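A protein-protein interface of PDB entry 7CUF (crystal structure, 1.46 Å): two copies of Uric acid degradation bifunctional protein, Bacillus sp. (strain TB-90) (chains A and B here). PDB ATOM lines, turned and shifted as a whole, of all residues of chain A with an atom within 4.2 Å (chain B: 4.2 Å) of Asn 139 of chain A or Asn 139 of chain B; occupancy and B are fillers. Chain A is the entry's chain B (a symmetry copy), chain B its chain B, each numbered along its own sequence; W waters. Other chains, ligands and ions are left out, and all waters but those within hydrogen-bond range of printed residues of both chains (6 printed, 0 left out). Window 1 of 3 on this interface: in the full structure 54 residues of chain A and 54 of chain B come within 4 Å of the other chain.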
ATOM      1  N   LYS A 136     -23.716 -18.099  -0.743  1.00  0.00           N
ATOM      2  CA  LYS A 136     -24.452 -17.018  -1.373  1.00  0.00           C
ATOM      3  C   LYS A 136     -25.268 -17.591  -2.526  1.00  0.00           C
ATOM      4  O   LYS A 136     -24.744 -18.336  -3.361  1.00  0.00           O
ATOM      5  CB  LYS A 136     -23.530 -15.925  -1.891  1.00  0.00           C
ATOM      6  CG  LYS A 136     -24.277 -14.704  -2.431  1.00  0.00           C
ATOM      7  CD  LYS A 136     -23.307 -13.544  -2.699  1.00  0.00           C
ATOM      8  CE  LYS A 136     -24.005 -12.191  -2.841  1.00  0.00           C
ATOM      9  NZ  LYS A 136     -23.530 -11.229  -1.765  1.00  0.00           N
ATOM     10  N   SER A 137     -26.549 -17.248  -2.577  1.00  0.00           N
ATOM     11  CA  SER A 137     -27.436 -17.773  -3.606  1.00  0.00           C
ATOM     12  C   SER A 137     -27.791 -16.695  -4.624  1.00  0.00           C
ATOM     13  O   SER A 137     -28.128 -15.560  -4.269  1.00  0.00           O
ATOM     14  CB  SER A 137     -28.727 -18.340  -3.041  1.00  0.00           C
ATOM     15  OG  SER A 137     -29.518 -18.785  -4.141  1.00  0.00           O
ATOM     16  N   ARG A 138     -27.769 -17.091  -5.899  1.00  0.00           N
ATOM     17  CA  ARG A 138     -28.117 -16.236  -7.018  1.00  0.00           C
ATOM     18  C   ARG A 138     -29.460 -16.654  -7.595  1.00  0.00           C
ATOM     19  O   ARG A 138     -29.811 -16.276  -8.713  1.00  0.00           O
ATOM     20  CB  ARG A 138     -27.027 -16.242  -8.072  1.00  0.00           C
ATOM     21  CG  ARG A 138     -25.776 -15.458  -7.624  1.00  0.00           C
ATOM     22  CD  ARG A 138     -24.816 -16.275  -6.827  1.00  0.00           C
ATOM     23  NE  ARG A 138     -24.006 -17.121  -7.703  1.00  0.00           N
ATOM     24  CZ  ARG A 138     -23.333 -18.177  -7.299  1.00  0.00           C
ATOM     25  NH1 ARG A 138     -23.332 -18.513  -6.027  1.00  0.00           N
ATOM     26  NH2 ARG A 138     -22.648 -18.891  -8.195  1.00  0.00           N
ATOM     27  N   ASN A 139     -30.237 -17.423  -6.828  1.00  0.00           N
ATOM     28  CA  ASN A 139     -31.575 -17.822  -7.261  1.00  0.00           C
ATOM     29  C   ASN A 139     -32.621 -16.872  -6.687  1.00  0.00           C
ATOM     30  O   ASN A 139     -32.397 -15.661  -6.652  1.00  0.00           O
ATOM     31  CB  ASN A 139     -31.786 -19.290  -6.864  1.00  0.00           C
ATOM     32  CG  ASN A 139     -30.761 -20.215  -7.555  1.00  0.00           C
ATOM     33  OD1 ASN A 139     -30.312 -19.907  -8.652  1.00  0.00           O
ATOM     34  ND2 ASN A 139     -30.419 -21.325  -6.947  1.00  0.00           N
ATOM     35  N   GLU A 140     -33.803 -17.368  -6.352  1.00  0.00           N
ATOM     36  CA  GLU A 140     -34.884 -16.458  -5.992  1.00  0.00           C
ATOM     37  C   GLU A 140     -34.639 -15.737  -4.649  1.00  0.00           C
ATOM     38  O   GLU A 140     -33.866 -16.169  -3.789  1.00  0.00           O
ATOM     39  CB  GLU A 140     -36.233 -17.191  -5.968  1.00  0.00           C
ATOM     40  CG  GLU A 140     -36.407 -18.215  -4.862  1.00  0.00           C
ATOM     41  CD  GLU A 140     -35.717 -19.541  -5.100  1.00  0.00           C
ATOM     42  OE1 GLU A 140     -35.086 -19.703  -6.161  1.00  0.00           O
ATOM     43  OE2 GLU A 140     -35.848 -20.439  -4.226  1.00  0.00           O
ATOM     44  N   TYR A 141     -35.342 -14.626  -4.466  1.00  0.00           N
ATOM     45  CA  TYR A 141     -35.115 -13.792  -3.302  1.00  0.00           C
ATOM     46  C   TYR A 141     -36.377 -12.984  -3.030  1.00  0.00           C
ATOM     47  O   TYR A 141     -37.188 -12.741  -3.929  1.00  0.00           O
ATOM     48  CB  TYR A 141     -33.917 -12.860  -3.517  1.00  0.00           C
ATOM     49  CG  TYR A 141     -34.001 -12.000  -4.767  1.00  0.00           C
ATOM     50  CD1 TYR A 141     -33.555 -12.463  -5.999  1.00  0.00           C
ATOM     51  CD2 TYR A 141     -34.559 -10.724  -4.717  1.00  0.00           C
ATOM     52  CE1 TYR A 141     -33.634 -11.681  -7.135  1.00  0.00           C
ATOM     53  CE2 TYR A 141     -34.646  -9.942  -5.855  1.00  0.00           C
ATOM     54  CZ  TYR A 141     -34.173 -10.413  -7.050  1.00  0.00           C
ATOM     55  OH  TYR A 141     -34.287  -9.639  -8.173  1.00  0.00           O
ATOM     56  N   GLY A 167     -37.234 -13.786  -9.140  1.00  0.00           N
ATOM     57  CA  GLY A 167     -36.164 -14.656  -9.632  1.00  0.00           C
ATOM     58  C   GLY A 167     -36.437 -16.138  -9.521  1.00  0.00           C
ATOM     59  O   GLY A 167     -35.490 -16.924  -9.506  1.00  0.00           O
ATOM     60  N   LYS B 136     -34.384 -24.124 -11.681  1.00  0.00           N
ATOM     61  CA  LYS B 136     -33.102 -23.878 -12.314  1.00  0.00           C
ATOM     62  C   LYS B 136     -32.211 -23.123 -11.335  1.00  0.00           C
ATOM     63  O   LYS B 136     -32.630 -22.122 -10.745  1.00  0.00           O
ATOM     64  CB  LYS B 136     -33.244 -23.078 -13.599  1.00  0.00           C
ATOM     65  CG  LYS B 136     -31.931 -22.924 -14.370  1.00  0.00           C
ATOM     66  CD  LYS B 136     -32.182 -22.336 -15.766  1.00  0.00           C
ATOM     67  CE  LYS B 136     -31.007 -22.532 -16.726  1.00  0.00           C
ATOM     68  NZ  LYS B 136     -31.430 -23.366 -17.923  1.00  0.00           N
ATOM     69  N   SER B 137     -30.983 -23.597 -11.159  1.00  0.00           N
ATOM     70  CA  SER B 137     -30.061 -22.985 -10.214  1.00  0.00           C
ATOM     71  C   SER B 137     -28.952 -22.232 -10.940  1.00  0.00           C
ATOM     72  O   SER B 137     -28.354 -22.733 -11.898  1.00  0.00           O
ATOM     73  CB  SER B 137     -29.418 -23.995  -9.278  1.00  0.00           C
ATOM     74  OG  SER B 137     -28.517 -23.283  -8.432  1.00  0.00           O
ATOM     75  N   ARG B 138     -28.646 -21.039 -10.424  1.00  0.00           N
ATOM     76  CA  ARG B 138     -27.593 -20.182 -10.935  1.00  0.00           C
ATOM     77  C   ARG B 138     -26.417 -20.169  -9.972  1.00  0.00           C
ATOM     78  O   ARG B 138     -25.552 -19.298 -10.044  1.00  0.00           O
ATOM     79  CB  ARG B 138     -28.110 -18.783 -11.208  1.00  0.00           C
ATOM     80  CG  ARG B 138     -29.015 -18.727 -12.456  1.00  0.00           C
ATOM     81  CD  ARG B 138     -30.443 -19.047 -12.169  1.00  0.00           C
ATOM     82  NE  ARG B 138     -31.126 -17.892 -11.588  1.00  0.00           N
ATOM     83  CZ  ARG B 138     -32.260 -17.956 -10.925  1.00  0.00           C
ATOM     84  NH1 ARG B 138     -32.875 -19.110 -10.778  1.00  0.00           N
ATOM     85  NH2 ARG B 138     -32.778 -16.837 -10.416  1.00  0.00           N
ATOM     86  N   ASN B 139     -26.361 -21.153  -9.070  1.00  0.00           N
ATOM     87  CA  ASN B 139     -25.236 -21.272  -8.144  1.00  0.00           C
ATOM     88  C   ASN B 139     -24.201 -22.248  -8.693  1.00  0.00           C
ATOM     89  O   ASN B 139     -23.922 -22.236  -9.892  1.00  0.00           O
ATOM     90  CB  ASN B 139     -25.792 -21.665  -6.768  1.00  0.00           C
ATOM     91  CG  ASN B 139     -26.756 -20.591  -6.219  1.00  0.00           C
ATOM     92  OD1 ASN B 139     -26.595 -19.418  -6.532  1.00  0.00           O
ATOM     93  ND2 ASN B 139     -27.711 -20.972  -5.407  1.00  0.00           N
ATOM     94  N   GLU B 140     -23.536 -23.005  -7.834  1.00  0.00           N
ATOM     95  CA  GLU B 140     -22.405 -23.797  -8.306  1.00  0.00           C
ATOM     96  C   GLU B 140     -22.832 -24.959  -9.229  1.00  0.00           C
ATOM     97  O   GLU B 140     -23.975 -25.426  -9.234  1.00  0.00           O
ATOM     98  CB  GLU B 140     -21.577 -24.327  -7.127  1.00  0.00           C
ATOM     99  CG  GLU B 140     -22.254 -25.373  -6.262  1.00  0.00           C
ATOM    100  CD  GLU B 140     -23.268 -24.832  -5.276  1.00  0.00           C
ATOM    101  OE1 GLU B 140     -23.459 -23.603  -5.232  1.00  0.00           O
ATOM    102  OE2 GLU B 140     -23.844 -25.653  -4.514  1.00  0.00           O
ATOM    103  N   TYR B 141     -21.872 -25.446 -10.007  1.00  0.00           N
ATOM    104  CA  TYR B 141     -22.171 -26.455 -11.005  1.00  0.00           C
ATOM    105  C   TYR B 141     -20.898 -27.234 -11.304  1.00  0.00           C
ATOM    106  O   TYR B 141     -19.783 -26.740 -11.107  1.00  0.00           O
ATOM    107  CB  TYR B 141     -22.723 -25.817 -12.285  1.00  0.00           C
ATOM    108  CG  TYR B 141     -21.840 -24.736 -12.884  1.00  0.00           C
ATOM    109  CD1 TYR B 141     -21.932 -23.412 -12.471  1.00  0.00           C
ATOM    110  CD2 TYR B 141     -20.886 -25.049 -13.849  1.00  0.00           C
ATOM    111  CE1 TYR B 141     -21.127 -22.430 -13.016  1.00  0.00           C
ATOM    112  CE2 TYR B 141     -20.074 -24.069 -14.391  1.00  0.00           C
ATOM    113  CZ  TYR B 141     -20.206 -22.768 -13.986  1.00  0.00           C
ATOM    114  OH  TYR B 141     -19.379 -21.811 -14.511  1.00  0.00           O
ATOM    115  N   GLY B 167     -18.191 -21.940  -9.472  1.00  0.00           N
ATOM    116  CA  GLY B 167     -19.246 -21.032  -9.016  1.00  0.00           C
ATOM    117  C   GLY B 167     -19.647 -21.187  -7.567  1.00  0.00           C
ATOM    118  O   GLY B 167     -20.756 -20.797  -7.206  1.00  0.00           O
HETATM  119  O   HOH W   1     -35.173 -20.036  -9.112  1.00  0.00           O
HETATM  120  O   HOH W   2     -29.195 -15.228 -10.926  1.00  0.00           O
HETATM  121  O   HOH W   3     -32.176 -14.021  -9.055  1.00  0.00           O
HETATM  122  O   HOH W   4     -24.816 -17.062 -10.959  1.00  0.00           O
HETATM  123  O   HOH W   5     -22.550 -20.004 -11.177  1.00  0.00           O
HETATM  124  O   HOH W   6     -22.405 -20.919  -4.521  1.00  0.00           O
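Of the 7 printed residues of chain A, 5 touch a printed residue of chain B.
Printed residues of chain A that touch a printed residue of chain B: Lys 136, Ser 137, Arg 138, Asn 139 and Gly 167.
Among the printed residues, 10 pairs touch across the chains.
Of the printed residues of chain B, Asn 139 of chain A touches Lys 136 (3.8 Å), Ser 137 (3.1 Å), Arg 138 (2.7 Å) and Asn 139 (3.1 Å).
Printed residues of chain A within 4 Å of Asn 139 of chain B: Lys 136 (3.8 Å), Ser 137 (3.1 Å), Arg 138 (2.7 Å) and Asn 139 (3.1 Å).
Of the printed residues of chain B, Arg 138 of chain A touches Arg 138 (3.5 Å), Asn 139 (2.7 Å) and Gly 167 (2.9 Å).
Of the printed residues of chain A, Ser 137 of chain B touches Asn 139.
Tyr 141 of chain A touches none of the printed residues of chain B.
Among the printed residues, pairs that only touch across the chains: Lys 136 of chain A with Asn 139 of chain B and Asn 139 of chain A with Lys 136 of chain B.
The backbone carbonyl oxygen (O) of Lys 136 of chain B sits at hydrogen-bond distance from the guanidinium group (NH1) of Arg 138 of chain B, at 3.0 Å.
The backbone NH of Asn 139 of chain B sits at hydrogen-bond distance from the side-chain hydroxyl of Ser 137 of chain B (3.1 Å).
The backbone carbonyl oxygen (O) of Lys 136 of chain A is in hydrogen-bond range of the guanidinium group (NH1) of Arg 138 of chain A, 3.0 Å away.
N of Asn 139 of chain A is in hydrogen-bond range of OG of Ser 137 of chain A (3.1 Å).
The side-chain hydroxyl (OG) of Ser 137 of chain B lies within hydrogen-bond range of the side-chain amide nitrogen (ND2) of Asn 139 of chain A (3.1 Å).
O of Arg 138 of chain B sits at hydrogen-bond distance from NH2 of Arg 138 of chain A (3.5 Å).
The backbone NH (N) of Arg 138 of chain B lies within hydrogen-bond range of the side-chain amide oxygen (OD1) of Asn 139 of chain A (2.7 Å).
The guanidinium group (NH2) of Arg 138 of chain B sits at hydrogen-bond distance from the backbone carbonyl oxygen (O) of Gly 167 of chain A (2.9 Å).
The side-chain amide nitrogen (ND2) of Asn 139 of chain B is in hydrogen-bond range of the side-chain hydroxyl (OG) of Ser 137 of chain A (3.1 Å).
The side-chain amide oxygen (OD1) of Asn 139 of chain B lies within hydrogen-bond range of the backbone NH (N) of Arg 138 of chain A, at 2.7 Å.
The side-chain amide nitrogen of Asn 139 of chain B lies close to the side-chain amide nitrogen of Asn 139 of chain A (3.1 Å).
The backbone carbonyl oxygen (O) of Gly 167 of chain B lies within hydrogen-bond range of the guanidinium group (NH2) of Arg 138 of chain A (2.9 Å).
Lys 136 of chain A touches Asn 139 of chain B, and with the chains exchanged Asn 139 of chain A touches Lys 136 of chain B.
Ser 137 of chain A touches Asn 139 of chain B, and with the chains exchanged Asn 139 of chain A touches Ser 137 of chain B.
Arg 138 of chain A touches Gly 167 of chain B, and with the chains exchanged Gly 167 of chain A touches Arg 138 of chain B.
Asn 139 of chain A touches its own counterpart, Asn 139 of chain B.
7 positions are printed for both chains.
Water W4 bridges the backbone carbonyl oxygen (O) of Arg 138 of chain B (2.5 Å) and the guanidinium group (NE) of Arg 138 of chain A (3.4 Å).
Water W2 lies within hydrogen-bond range of the backbone carbonyl oxygen (O) of Arg 138 of chain A (2.5 Å) and the guanidinium group (NE) of Arg 138 of chain B (3.4 Å).
Water W5 lies within hydrogen-bond range of the backbone carbonyl oxygen (O) of Asn 139 of chain B (2.9 Å), the guanidinium group (NH2) of Arg 138 of chain A (3.2 Å) and the backbone carbonyl oxygen (O) of Arg 138 of chain B (3.3 Å).
Water W3 lies within hydrogen-bond range of the backbone carbonyl oxygen (O) of Asn 139 of chain A (2.9 Å), the guanidinium group (NH2) of Arg 138 of chain B (3.2 Å) and the backbone carbonyl oxygen (O) of Arg 138 of chain A (3.3 Å).
Water W6 lies within hydrogen-bond range of OE1 of Glu 140 of chain B, NH1 of Arg 138 of chain A and O of Gly 167 of chain B.
Water W1 lies within hydrogen-bond range of the side-chain carboxylate of Glu 140 of chain A (3.0 Å), the guanidinium group of Arg 138 of chain B (3.0 Å) and the backbone carbonyl oxygen of Gly 167 of chain A (3.2 Å).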
